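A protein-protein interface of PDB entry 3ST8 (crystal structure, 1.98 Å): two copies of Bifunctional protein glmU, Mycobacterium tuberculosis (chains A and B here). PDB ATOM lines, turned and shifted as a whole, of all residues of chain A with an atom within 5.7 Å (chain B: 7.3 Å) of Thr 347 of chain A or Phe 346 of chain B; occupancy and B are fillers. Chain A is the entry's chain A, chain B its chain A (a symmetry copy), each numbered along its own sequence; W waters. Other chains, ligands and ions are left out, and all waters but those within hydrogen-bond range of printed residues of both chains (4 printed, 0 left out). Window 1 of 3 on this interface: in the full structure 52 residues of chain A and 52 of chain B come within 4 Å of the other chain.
CD2 of His 331 of chain A touches CB of Pro 345 of chain B, at 3.97 Å. His 331 of chain A touches Phe 346 of chain B (CB to CE2, 3.96 Å). Phe 346 of chain A touches Phe 346 of chain B. CE2 of Phe 346 of chain B touches O of Thr 347 of chain A (3.6 Å). CD2 of Tyr 348 of chain A touches CB of Ala 363 of chain B, at 3.6 Å. Phe 364 of chain A touches Phe 364 of chain B (C to CE2, 3.4 Å). Phe 364 of chain A touches Leu 381 of chain B. Val 365 of chain A touches Phe 364 of chain B (O to CE2, 3.5 Å). Glu 366 of chain A touches Ala 363 of chain B (OE1 to CB, 3.7 Å). N of Glu 366 of chain A touches CE2 of Phe 364 of chain B (3.9 Å).
Water W4 bridges the side-chain hydroxyl of Tyr 348 of chain A (2.6 Å) and the backbone carbonyl oxygen of Gly 344 of chain B (3.0 Å). Water W2 bridges OE1 of Glu 366 of chain A and N of Ala 363 of chain B. Water W3 bridges the side-chain carboxylate of Glu 366 of chain A (2.7 Å) and the backbone carbonyl oxygen of Ala 363 of chain B (2.9 Å). Water W1 lies within hydrogen-bond range of the side-chain carboxylate of Asp 313 of chain B, the guanidinium group of Arg 329 of chain A and the guanidinium group of Arg 329 of chain B.
ND1 of His 331 of chain A is in hydrogen-bond range of NE of Arg 329 of chain B (2.9 Å).
Of the 18 printed residues of chain A, 8 touch a printed residue of chain B. Along chain A the printed residues that touch a printed residue of chain B span positions 329 to 366. Among the printed residues, no Asp or Glu carboxylate lies within 4 Å of a Lys or Arg side-chain nitrogen of the other chain.
Of the printed residues of chain A, Phe 346 of chain B touches Arg 329, His 331, Phe 346 and Thr 347. Of the printed residues of chain B, Arg 329 of chain A touches Phe 346. Printed residues of chain B within 4 Å of Glu 366 of chain A: Ala 363 and Phe 364. Printed residues of chain B within 4 Å of Phe 346 of chain A: Phe 346 (3.997 Å) and Phe 364 (3.3 Å). Printed residues of chain A within 4 Å of Pro 345 of chain B: His 331 and Tyr 348. Gly 344 of chain B touches none of the printed residues of chain A. The nearest printed residue of chain A that does not touch Phe 346 of chain B is Tyr 348 of chain A (4.2 Å). The nearest printed residue of chain B that does not touch Tyr 348 of chain A is Phe 364 of chain B (4.1 Å).
Arg 329 of chain A touches Phe 346 of chain B, but with the chains exchanged Phe 346 of chain A does not touch Arg 329 of chain B (7.4 Å). His 331 of chain A touches Val 328 of chain B, but with the chains exchanged Val 328 of chain A does not touch His 331 of chain B (16.2 Å). Tyr 348 of chain A touches Ala 363 of chain B, but with the chains exchanged Ala 363 of chain A does not touch Tyr 348 of chain B (13.8 Å). Val 365 of chain A touches Phe 364 of chain B, but with the chains exchanged Phe 364 of chain A does not touch Val 365 of chain B (8.1 Å). Positions printed for both chains: 328, 329, 330, 331, 343, 344, 345, 346, 347, 348, 361, 362, 363, 364, 365 and 366. Of the 15 pairs that touch across the chains among the printed residues, 2 have their exchanged pair printed and touching as well.
N of Thr 347 of chain A lies within hydrogen-bond range of O of Arg 329 of chain A (3.4 Å). O of His 331 of chain A lies within hydrogen-bond range of N of Leu 349 of chain A, 2.9 Å away. The backbone NH (N) of Phe 364 of chain A lies within hydrogen-bond range of the backbone carbonyl oxygen (O) of Phe 346 of chain A (2.8 Å). OD2 of Asp 313 of chain B is in salt-bridge range of NH1 of Arg 329 of chain B (2.8 Å). The backbone carbonyl oxygen (O) of Val 328 of chain B is in hydrogen-bond range of the side-chain hydroxyl (OG1) of Thr 330 of chain B. The backbone carbonyl oxygen (O) of Ala 363 of chain B is in hydrogen-bond range of the backbone NH (N) of Leu 381 of chain B (3.0 Å).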
ATOM      1  N   VAL A 328     -22.075  27.780   4.548  1.00  0.00           N
ATOM      2  CA  VAL A 328     -23.460  28.309   4.683  1.00  0.00           C
ATOM      3  C   VAL A 328     -24.351  27.435   3.849  1.00  0.00           C
ATOM      4  O   VAL A 328     -23.983  27.098   2.715  1.00  0.00           O
ATOM      5  CB  VAL A 328     -23.493  29.687   3.999  1.00  0.00           C
ATOM      6  CG1 VAL A 328     -24.873  30.292   4.025  1.00  0.00           C
ATOM      7  CG2 VAL A 328     -22.522  30.657   4.883  1.00  0.00           C
ATOM      8  N   ARG A 329     -25.553  27.091   4.365  1.00  0.00           N
ATOM      9  CA  ARG A 329     -26.524  26.265   3.584  1.00  0.00           C
ATOM     10  C   ARG A 329     -25.813  25.131   2.909  1.00  0.00           C
ATOM     11  O   ARG A 329     -26.028  24.866   1.711  1.00  0.00           O
ATOM     12  CB  ARG A 329     -27.244  27.167   2.573  1.00  0.00           C
ATOM     13  CG  ARG A 329     -28.246  28.107   3.328  1.00  0.00           C
ATOM     14  CD  ARG A 329     -29.259  28.859   2.339  1.00  0.00           C
ATOM     15  NE  ARG A 329     -30.127  29.678   3.210  1.00  0.00           N
ATOM     16  CZ  ARG A 329     -31.051  29.195   4.039  1.00  0.00           C
ATOM     17  NH1 ARG A 329     -31.366  27.854   4.069  1.00  0.00           N
ATOM     18  NH2 ARG A 329     -31.675  30.062   4.858  1.00  0.00           N
ATOM     19  N   THR A 330     -25.035  24.361   3.669  1.00  0.00           N
ATOM     20  CA  THR A 330     -24.198  23.317   2.976  1.00  0.00           C
ATOM     21  C   THR A 330     -24.605  21.950   3.639  1.00  0.00           C
ATOM     22  O   THR A 330     -24.843  21.878   4.863  1.00  0.00           O
ATOM     23  CB  THR A 330     -22.733  23.613   3.298  1.00  0.00           C
ATOM     24  OG1 THR A 330     -22.343  24.714   2.431  1.00  0.00           O
ATOM     25  CG2 THR A 330     -21.765  22.390   2.941  1.00  0.00           C
ATOM     26  N   HIS A 331     -24.630  20.917   2.840  1.00  0.00           N
ATOM     27  CA  HIS A 331     -24.888  19.538   3.342  1.00  0.00           C
ATOM     28  C   HIS A 331     -23.600  18.750   2.993  1.00  0.00           C
ATOM     29  O   HIS A 331     -23.206  18.585   1.860  1.00  0.00           O
ATOM     30  CB  HIS A 331     -26.096  18.966   2.554  1.00  0.00           C
ATOM     31  CG  HIS A 331     -26.695  17.727   3.173  1.00  0.00           C
ATOM     32  ND1 HIS A 331     -27.515  17.774   4.303  1.00  0.00           N
ATOM     33  CD2 HIS A 331     -26.510  16.420   2.876  1.00  0.00           C
ATOM     34  CE1 HIS A 331     -27.834  16.524   4.651  1.00  0.00           C
ATOM     35  NE2 HIS A 331     -27.247  15.688   3.791  1.00  0.00           N
ATOM     36  N   GLY A 332     -22.869  18.339   4.014  1.00  0.00           N
ATOM     37  CA  GLY A 332     -21.580  17.757   3.694  1.00  0.00           C
ATOM     38  C   GLY A 332     -21.112  16.681   4.665  1.00  0.00           C
ATOM     39  O   GLY A 332     -21.489  16.715   5.836  1.00  0.00           O
ATOM     40  N   VAL A 343     -17.774  28.206   1.404  1.00  0.00           N
ATOM     41  CA  VAL A 343     -18.588  27.111   0.876  1.00  0.00           C
ATOM     42  C   VAL A 343     -20.055  27.515   1.024  1.00  0.00           C
ATOM     43  O   VAL A 343     -20.463  27.991   2.059  1.00  0.00           O
ATOM     44  CB  VAL A 343     -18.273  25.785   1.654  1.00  0.00           C
ATOM     45  CG1 VAL A 343     -19.178  24.613   1.107  1.00  0.00           C
ATOM     46  CG2 VAL A 343     -16.783  25.369   1.445  1.00  0.00           C
ATOM     47  N   GLY A 344     -20.839  27.347  -0.054  1.00  0.00           N
ATOM     48  CA  GLY A 344     -22.290  27.616   0.003  1.00  0.00           C
ATOM     49  C   GLY A 344     -22.628  28.974  -0.663  1.00  0.00           C
ATOM     50  O   GLY A 344     -21.746  29.698  -1.138  1.00  0.00           O
ATOM     51  N   PRO A 345     -23.916  29.356  -0.664  1.00  0.00           N
ATOM     52  CA  PRO A 345     -25.053  28.608  -0.102  1.00  0.00           C
ATOM     53  C   PRO A 345     -25.417  27.501  -1.089  1.00  0.00           C
ATOM     54  O   PRO A 345     -25.147  27.635  -2.307  1.00  0.00           O
ATOM     55  CB  PRO A 345     -26.181  29.697  -0.053  1.00  0.00           C
ATOM     56  CG  PRO A 345     -25.886  30.529  -1.242  1.00  0.00           C
ATOM     57  CD  PRO A 345     -24.308  30.674  -1.231  1.00  0.00           C
ATOM     58  N   PHE A 346     -26.090  26.440  -0.622  1.00  0.00           N
ATOM     59  CA  PHE A 346     -26.591  25.353  -1.459  1.00  0.00           C
ATOM     60  C   PHE A 346     -25.463  24.539  -2.086  1.00  0.00           C
ATOM     61  O   PHE A 346     -25.380  24.435  -3.320  1.00  0.00           O
ATOM     62  CB  PHE A 346     -27.562  25.816  -2.573  1.00  0.00           C
ATOM     63  CG  PHE A 346     -28.648  26.766  -2.057  1.00  0.00           C
ATOM     64  CD1 PHE A 346     -29.659  26.305  -1.222  1.00  0.00           C
ATOM     65  CD2 PHE A 346     -28.581  28.129  -2.423  1.00  0.00           C
ATOM     66  CE1 PHE A 346     -30.750  27.219  -0.722  1.00  0.00           C
ATOM     67  CE2 PHE A 346     -29.546  29.032  -2.000  1.00  0.00           C
ATOM     68  CZ  PHE A 346     -30.650  28.591  -1.093  1.00  0.00           C
ATOM     69  N   THR A 347     -24.668  23.899  -1.223  1.00  0.00           N
ATOM     70  CA  THR A 347     -23.509  23.151  -1.738  1.00  0.00           C
ATOM     71  C   THR A 347     -23.585  21.773  -1.117  1.00  0.00           C
ATOM     72  O   THR A 347     -23.918  21.688   0.037  1.00  0.00           O
ATOM     73  CB  THR A 347     -22.191  23.865  -1.253  1.00  0.00           C
ATOM     74  OG1 THR A 347     -22.272  25.184  -1.847  1.00  0.00           O
ATOM     75  CG2 THR A 347     -20.965  23.183  -1.830  1.00  0.00           C
ATOM     76  N   TYR A 348     -23.165  20.728  -1.875  1.00  0.00           N
ATOM     77  CA  TYR A 348     -23.286  19.374  -1.390  1.00  0.00           C
ATOM     78  C   TYR A 348     -21.834  18.791  -1.456  1.00  0.00           C
ATOM     79  O   TYR A 348     -21.253  18.726  -2.500  1.00  0.00           O
ATOM     80  CB  TYR A 348     -24.190  18.637  -2.368  1.00  0.00           C
ATOM     81  CG  TYR A 348     -24.391  17.139  -2.048  1.00  0.00           C
ATOM     82  CD1 TYR A 348     -24.211  16.653  -0.743  1.00  0.00           C
ATOM     83  CD2 TYR A 348     -24.782  16.251  -3.074  1.00  0.00           C
ATOM     84  CE1 TYR A 348     -24.513  15.226  -0.443  1.00  0.00           C
ATOM     85  CE2 TYR A 348     -25.083  14.891  -2.810  1.00  0.00           C
ATOM     86  CZ  TYR A 348     -24.957  14.431  -1.511  1.00  0.00           C
ATOM     87  OH  TYR A 348     -25.207  13.121  -1.315  1.00  0.00           O
ATOM     88  N   LEU A 349     -21.284  18.441  -0.308  1.00  0.00           N
ATOM     89  CA  LEU A 349     -19.905  17.841  -0.245  1.00  0.00           C
ATOM     90  C   LEU A 349     -20.083  16.348   0.102  1.00  0.00           C
ATOM     91  O   LEU A 349     -20.695  16.025   1.158  1.00  0.00           O
ATOM     92  CB  LEU A 349     -19.114  18.488   0.890  1.00  0.00           C
ATOM     93  CG  LEU A 349     -19.094  20.054   0.775  1.00  0.00           C
ATOM     94  CD1 LEU A 349     -18.166  20.590   1.850  1.00  0.00           C
ATOM     95  CD2 LEU A 349     -18.527  20.486  -0.574  1.00  0.00           C
ATOM     96  N   LEU A 361     -16.343  26.859  -3.023  1.00  0.00           N
ATOM     97  CA  LEU A 361     -17.298  25.957  -3.645  1.00  0.00           C
ATOM     98  C   LEU A 361     -18.655  26.681  -3.478  1.00  0.00           C
ATOM     99  O   LEU A 361     -19.123  26.852  -2.349  1.00  0.00           O
ATOM    100  CB  LEU A 361     -17.335  24.599  -2.934  1.00  0.00           C
ATOM    101  CG  LEU A 361     -15.934  23.883  -3.068  1.00  0.00           C
ATOM    102  CD1 LEU A 361     -16.113  22.612  -2.253  1.00  0.00           C
ATOM    103  CD2 LEU A 361     -15.521  23.475  -4.472  1.00  0.00           C
ATOM    104  N   GLY A 362     -19.202  27.128  -4.611  1.00  0.00           N
ATOM    105  CA  GLY A 362     -20.259  28.108  -4.618  1.00  0.00           C
ATOM    106  C   GLY A 362     -21.638  27.437  -4.701  1.00  0.00           C
ATOM    107  O   GLY A 362     -21.809  26.209  -4.381  1.00  0.00           O
ATOM    108  N   ALA A 363     -22.645  28.205  -5.109  1.00  0.00           N
ATOM    109  CA  ALA A 363     -24.040  27.707  -5.069  1.00  0.00           C
ATOM    110  C   ALA A 363     -24.264  26.662  -6.159  1.00  0.00           C
ATOM    111  O   ALA A 363     -23.891  26.825  -7.340  1.00  0.00           O
ATOM    112  CB  ALA A 363     -25.036  28.930  -5.213  1.00  0.00           C
ATOM    113  N   PHE A 364     -25.021  25.644  -5.767  1.00  0.00           N
ATOM    114  CA  PHE A 364     -25.404  24.563  -6.678  1.00  0.00           C
ATOM    115  C   PHE A 364     -24.185  23.807  -7.190  1.00  0.00           C
ATOM    116  O   PHE A 364     -24.098  23.440  -8.375  1.00  0.00           O
ATOM    117  CB  PHE A 364     -26.345  25.050  -7.802  1.00  0.00           C
ATOM    118  CG  PHE A 364     -27.297  26.130  -7.284  1.00  0.00           C
ATOM    119  CD1 PHE A 364     -28.135  25.875  -6.150  1.00  0.00           C
ATOM    120  CD2 PHE A 364     -27.294  27.392  -7.892  1.00  0.00           C
ATOM    121  CE1 PHE A 364     -28.986  26.932  -5.572  1.00  0.00           C
ATOM    122  CE2 PHE A 364     -28.158  28.473  -7.363  1.00  0.00           C
ATOM    123  CZ  PHE A 364     -28.954  28.241  -6.212  1.00  0.00           C
ATOM    124  N   VAL A 365     -23.255  23.560  -6.275  1.00  0.00           N
ATOM    125  CA  VAL A 365     -22.039  22.801  -6.636  1.00  0.00           C
ATOM    126  C   VAL A 365     -22.065  21.528  -5.763  1.00  0.00           C
ATOM    127  O   VAL A 365     -22.399  21.558  -4.590  1.00  0.00           O
ATOM    128  CB  VAL A 365     -20.785  23.583  -6.233  1.00  0.00           C
ATOM    129  CG1 VAL A 365     -19.429  22.694  -6.393  1.00  0.00           C
ATOM    130  CG2 VAL A 365     -20.699  24.789  -7.140  1.00  0.00           C
ATOM    131  N   GLU A 366     -21.667  20.441  -6.419  1.00  0.00           N
ATOM    132  CA  GLU A 366     -21.585  19.163  -5.723  1.00  0.00           C
ATOM    133  C   GLU A 366     -20.133  18.667  -5.986  1.00  0.00           C
ATOM    134  O   GLU A 366     -19.674  18.681  -7.159  1.00  0.00           O
ATOM    135  CB  GLU A 366     -22.552  18.115  -6.310  1.00  0.00           C
ATOM    136  CG  GLU A 366     -22.252  16.678  -5.793  1.00  0.00           C
ATOM    137  CD  GLU A 366     -23.285  15.630  -6.248  1.00  0.00           C
ATOM    138  OE1 GLU A 366     -24.416  16.014  -6.697  1.00  0.00           O
ATOM    139  OE2 GLU A 366     -22.966  14.397  -6.179  1.00  0.00           O
ATOM    140  N   ASP B 313     -34.847  19.685   6.713  1.00  0.00           N
ATOM    141  CA  ASP B 313     -35.233  20.778   5.872  1.00  0.00           C
ATOM    142  C   ASP B 313     -35.902  20.360   4.590  1.00  0.00           C
ATOM    143  O   ASP B 313     -35.538  20.757   3.502  1.00  0.00           O
ATOM    144  CB  ASP B 313     -34.019  21.626   5.551  1.00  0.00           C
ATOM    145  CG  ASP B 313     -33.519  22.397   6.780  1.00  0.00           C
ATOM    146  OD1 ASP B 313     -34.210  22.440   7.884  1.00  0.00           O
ATOM    147  OD2 ASP B 313     -32.425  22.983   6.650  1.00  0.00           O
ATOM    148  N   VAL B 328     -34.236  13.998   1.459  1.00  0.00           N
ATOM    149  CA  VAL B 328     -33.403  14.891   2.309  1.00  0.00           C
ATOM    150  C   VAL B 328     -33.357  16.231   1.632  1.00  0.00           C
ATOM    151  O   VAL B 328     -33.176  16.286   0.407  1.00  0.00           O
ATOM    152  CB  VAL B 328     -31.959  14.363   2.254  1.00  0.00           C
ATOM    153  CG1 VAL B 328     -31.013  15.235   3.039  1.00  0.00           C
ATOM    154  CG2 VAL B 328     -31.982  12.899   2.978  1.00  0.00           C
ATOM    155  N   ARG B 329     -33.469  17.331   2.410  1.00  0.00           N
ATOM    156  CA  ARG B 329     -33.383  18.705   1.826  1.00  0.00           C
ATOM    157  C   ARG B 329     -34.183  18.780   0.560  1.00  0.00           C
ATOM    158  O   ARG B 329     -33.709  19.308  -0.463  1.00  0.00           O
ATOM    159  CB  ARG B 329     -31.908  19.054   1.589  1.00  0.00           C
ATOM    160  CG  ARG B 329     -31.200  19.309   2.964  1.00  0.00           C
ATOM    161  CD  ARG B 329     -29.752  19.977   2.804  1.00  0.00           C
ATOM    162  NE  ARG B 329     -29.245  20.156   4.180  1.00  0.00           N
ATOM    163  CZ  ARG B 329     -29.723  21.032   5.061  1.00  0.00           C
ATOM    164  NH1 ARG B 329     -30.684  21.956   4.716  1.00  0.00           N
ATOM    165  NH2 ARG B 329     -29.237  20.989   6.316  1.00  0.00           N
ATOM    166  N   THR B 330     -35.446  18.362   0.613  1.00  0.00           N
ATOM    167  CA  THR B 330     -36.211  18.287  -0.684  1.00  0.00           C
ATOM    168  C   THR B 330     -37.481  19.190  -0.471  1.00  0.00           C
ATOM    169  O   THR B 330     -38.075  19.209   0.627  1.00  0.00           O
ATOM    170  CB  THR B 330     -36.653  16.837  -0.876  1.00  0.00           C
ATOM    171  OG1 THR B 330     -35.483  16.118  -1.353  1.00  0.00           O
ATOM    172  CG2 THR B 330     -37.773  16.680  -2.007  1.00  0.00           C
ATOM    173  N   HIS B 331     -37.880  19.863  -1.516  1.00  0.00           N
ATOM    174  CA  HIS B 331     -39.132  20.674  -1.502  1.00  0.00           C
ATOM    175  C   HIS B 331     -40.025  20.028  -2.591  1.00  0.00           C
ATOM    176  O   HIS B 331     -39.718  19.977  -3.761  1.00  0.00           O
ATOM    177  CB  HIS B 331     -38.759  22.125  -1.905  1.00  0.00           C
ATOM    178  CG  HIS B 331     -39.840  23.135  -1.607  1.00  0.00           C
ATOM    179  ND1 HIS B 331     -40.088  23.608  -0.316  1.00  0.00           N
ATOM    180  CD2 HIS B 331     -40.783  23.676  -2.412  1.00  0.00           C
ATOM    181  CE1 HIS B 331     -41.138  24.434  -0.358  1.00  0.00           C
ATOM    182  NE2 HIS B 331     -41.566  24.500  -1.622  1.00  0.00           N
ATOM    183  N   VAL B 343     -33.810  10.689  -2.716  1.00  0.00           N
ATOM    184  CA  VAL B 343     -34.119  12.016  -3.248  1.00  0.00           C
ATOM    185  C   VAL B 343     -33.363  13.039  -2.401  1.00  0.00           C
ATOM    186  O   VAL B 343     -33.371  12.966  -1.192  1.00  0.00           O
ATOM    187  CB  VAL B 343     -35.669  12.262  -3.205  1.00  0.00           C
ATOM    188  CG1 VAL B 343     -35.998  13.709  -3.745  1.00  0.00           C
ATOM    189  CG2 VAL B 343     -36.411  11.237  -4.118  1.00  0.00           C
ATOM    190  N   GLY B 344     -32.674  13.983  -3.065  1.00  0.00           N
ATOM    191  CA  GLY B 344     -31.983  15.075  -2.350  1.00  0.00           C
ATOM    192  C   GLY B 344     -30.458  14.811  -2.277  1.00  0.00           C
ATOM    193  O   GLY B 344     -29.955  13.788  -2.755  1.00  0.00           O
ATOM    194  N   PRO B 345     -29.707  15.719  -1.634  1.00  0.00           N
ATOM    195  CA  PRO B 345     -30.183  16.956  -0.991  1.00  0.00           C
ATOM    196  C   PRO B 345     -30.426  17.988  -2.090  1.00  0.00           C
ATOM    197  O   PRO B 345     -29.798  17.911  -3.173  1.00  0.00           O
ATOM    198  CB  PRO B 345     -28.955  17.371  -0.107  1.00  0.00           C
ATOM    199  CG  PRO B 345     -27.800  16.921  -0.918  1.00  0.00           C
ATOM    200  CD  PRO B 345     -28.244  15.504  -1.472  1.00  0.00           C
ATOM    201  N   PHE B 346     -31.263  19.001  -1.825  1.00  0.00           N
ATOM    202  CA  PHE B 346     -31.520  20.113  -2.736  1.00  0.00           C
ATOM    203  C   PHE B 346     -32.238  19.667  -4.006  1.00  0.00           C
ATOM    204  O   PHE B 346     -31.722  19.869  -5.118  1.00  0.00           O
ATOM    205  CB  PHE B 346     -30.250  20.911  -3.124  1.00  0.00           C
ATOM    206  CG  PHE B 346     -29.385  21.274  -1.914  1.00  0.00           C
ATOM    207  CD1 PHE B 346     -29.817  22.214  -0.985  1.00  0.00           C
ATOM    208  CD2 PHE B 346     -28.149  20.610  -1.745  1.00  0.00           C
ATOM    209  CE1 PHE B 346     -28.969  22.602   0.201  1.00  0.00           C
ATOM    210  CE2 PHE B 346     -27.314  20.911  -0.678  1.00  0.00           C
ATOM    211  CZ  PHE B 346     -27.735  21.906   0.356  1.00  0.00           C
ATOM    212  N   THR B 347     -33.457  19.151  -3.826  1.00  0.00           N
ATOM    213  CA  THR B 347     -34.191  18.626  -4.989  1.00  0.00           C
ATOM    214  C   THR B 347     -35.564  19.260  -4.945  1.00  0.00           C
ATOM    215  O   THR B 347     -36.100  19.379  -3.873  1.00  0.00           O
ATOM    216  CB  THR B 347     -34.336  17.065  -4.832  1.00  0.00           C
ATOM    217  OG1 THR B 347     -32.968  16.590  -4.814  1.00  0.00           O
ATOM    218  CG2 THR B 347     -35.008  16.461  -6.050  1.00  0.00           C
ATOM    219  N   TYR B 348     -36.150  19.553  -6.134  1.00  0.00           N
ATOM    220  CA  TYR B 348     -37.421  20.237  -6.179  1.00  0.00           C
ATOM    221  C   TYR B 348     -38.353  19.300  -7.017  1.00  0.00           C
ATOM    222  O   TYR B 348     -38.079  19.024  -8.148  1.00  0.00           O
ATOM    223  CB  TYR B 348     -37.189  21.545  -6.921  1.00  0.00           C
ATOM    224  CG  TYR B 348     -38.460  22.397  -7.126  1.00  0.00           C
ATOM    225  CD1 TYR B 348     -39.568  22.251  -6.275  1.00  0.00           C
ATOM    226  CD2 TYR B 348     -38.503  23.352  -8.166  1.00  0.00           C
ATOM    227  CE1 TYR B 348     -40.738  23.158  -6.432  1.00  0.00           C
ATOM    228  CE2 TYR B 348     -39.603  24.232  -8.328  1.00  0.00           C
ATOM    229  CZ  TYR B 348     -40.668  24.119  -7.452  1.00  0.00           C
ATOM    230  OH  TYR B 348     -41.711  24.943  -7.672  1.00  0.00           O
ATOM    231  N   LEU B 361     -33.125  10.927  -7.506  1.00  0.00           N
ATOM    232  CA  LEU B 361     -33.186  12.296  -7.990  1.00  0.00           C
ATOM    233  C   LEU B 361     -32.225  13.064  -7.051  1.00  0.00           C
ATOM    234  O   LEU B 361     -32.500  13.176  -5.853  1.00  0.00           O
ATOM    235  CB  LEU B 361     -34.604  12.870  -7.877  1.00  0.00           C
ATOM    236  CG  LEU B 361     -35.589  12.054  -8.802  1.00  0.00           C
ATOM    237  CD1 LEU B 361     -36.941  12.688  -8.515  1.00  0.00           C
ATOM    238  CD2 LEU B 361     -35.343  12.154 -10.298  1.00  0.00           C
ATOM    239  N   GLY B 362     -31.108  13.512  -7.628  1.00  0.00           N
ATOM    240  CA  GLY B 362     -29.962  13.929  -6.858  1.00  0.00           C
ATOM    241  C   GLY B 362     -29.967  15.449  -6.636  1.00  0.00           C
ATOM    242  O   GLY B 362     -31.036  16.143  -6.753  1.00  0.00           O
ATOM    243  N   ALA B 363     -28.803  16.000  -6.303  1.00  0.00           N
ATOM    244  CA  ALA B 363     -28.728  17.426  -5.908  1.00  0.00           C
ATOM    245  C   ALA B 363     -28.919  18.327  -7.125  1.00  0.00           C
ATOM    246  O   ALA B 363     -28.322  18.141  -8.206  1.00  0.00           O
ATOM    247  CB  ALA B 363     -27.342  17.697  -5.188  1.00  0.00           C
ATOM    248  N   PHE B 364     -29.654  19.404  -6.874  1.00  0.00           N
ATOM    249  CA  PHE B 364     -29.910  20.426  -7.892  1.00  0.00           C
ATOM    250  C   PHE B 364     -30.673  19.853  -9.079  1.00  0.00           C
ATOM    251  O   PHE B 364     -30.391  20.172 -10.247  1.00  0.00           O
ATOM    252  CB  PHE B 364     -28.628  21.189  -8.292  1.00  0.00           C
ATOM    253  CG  PHE B 364     -27.707  21.374  -7.084  1.00  0.00           C
ATOM    254  CD1 PHE B 364     -28.190  22.010  -5.894  1.00  0.00           C
ATOM    255  CD2 PHE B 364     -26.405  20.857  -7.132  1.00  0.00           C
ATOM    256  CE1 PHE B 364     -27.352  22.109  -4.684  1.00  0.00           C
ATOM    257  CE2 PHE B 364     -25.520  20.965  -5.948  1.00  0.00           C
ATOM    258  CZ  PHE B 364     -26.008  21.551  -4.753  1.00  0.00           C
ATOM    259  N   VAL B 365     -31.656  19.020  -8.763  1.00  0.00           N
ATOM    260  CA  VAL B 365     -32.496  18.423  -9.822  1.00  0.00           C
ATOM    261  C   VAL B 365     -33.932  18.918  -9.546  1.00  0.00           C
ATOM    262  O   VAL B 365     -34.388  18.976  -8.417  1.00  0.00           O
ATOM    263  CB  VAL B 365     -32.524  16.898  -9.685  1.00  0.00           C
ATOM    264  CG1 VAL B 365     -33.617  16.211 -10.678  1.00  0.00           C
ATOM    265  CG2 VAL B 365     -31.144  16.393 -10.038  1.00  0.00           C
ATOM    266  N   GLU B 366     -34.595  19.232 -10.657  1.00  0.00           N
ATOM    267  CA  GLU B 366     -35.984  19.668 -10.574  1.00  0.00           C
ATOM    268  C   GLU B 366     -36.749  18.723 -11.547  1.00  0.00           C
ATOM    269  O   GLU B 366     -36.303  18.536 -12.710  1.00  0.00           O
ATOM    270  CB  GLU B 366     -36.173  21.112 -11.078  1.00  0.00           C
ATOM    271  CG  GLU B 366     -37.672  21.474 -11.290  1.00  0.00           C
ATOM    272  CD  GLU B 366     -37.905  22.951 -11.656  1.00  0.00           C
ATOM    273  OE1 GLU B 366     -36.979  23.805 -11.451  1.00  0.00           O
ATOM    274  OE2 GLU B 366     -39.024  23.276 -12.178  1.00  0.00           O
ATOM    275  N   LEU B 381     -27.979  18.248 -11.139  1.00  0.00           N
ATOM    276  CA  LEU B 381     -28.003  19.578 -11.903  1.00  0.00           C
ATOM    277  C   LEU B 381     -28.836  19.436 -13.153  1.00  0.00           C
ATOM    278  O   LEU B 381     -28.455  19.897 -14.223  1.00  0.00           O
ATOM    279  CB  LEU B 381     -26.550  19.966 -12.323  1.00  0.00           C
ATOM    280  CG  LEU B 381     -25.855  20.459 -11.000  1.00  0.00           C
ATOM    281  CD1 LEU B 381     -24.323  20.302 -11.258  1.00  0.00           C
ATOM    282  CD2 LEU B 381     -26.134  22.039 -10.688  1.00  0.00           C
HETATM  283  O   HOH W   1     -32.673  24.665   3.939  1.00  0.00           O
HETATM  284  O   HOH W   2     -26.401  14.291  -6.381  1.00  0.00           O
HETATM  285  O   HOH W   3     -25.450  17.847  -8.447  1.00  0.00           O
HETATM  286  O   HOH W   4     -27.642  12.214  -1.787  1.00  0.00           O
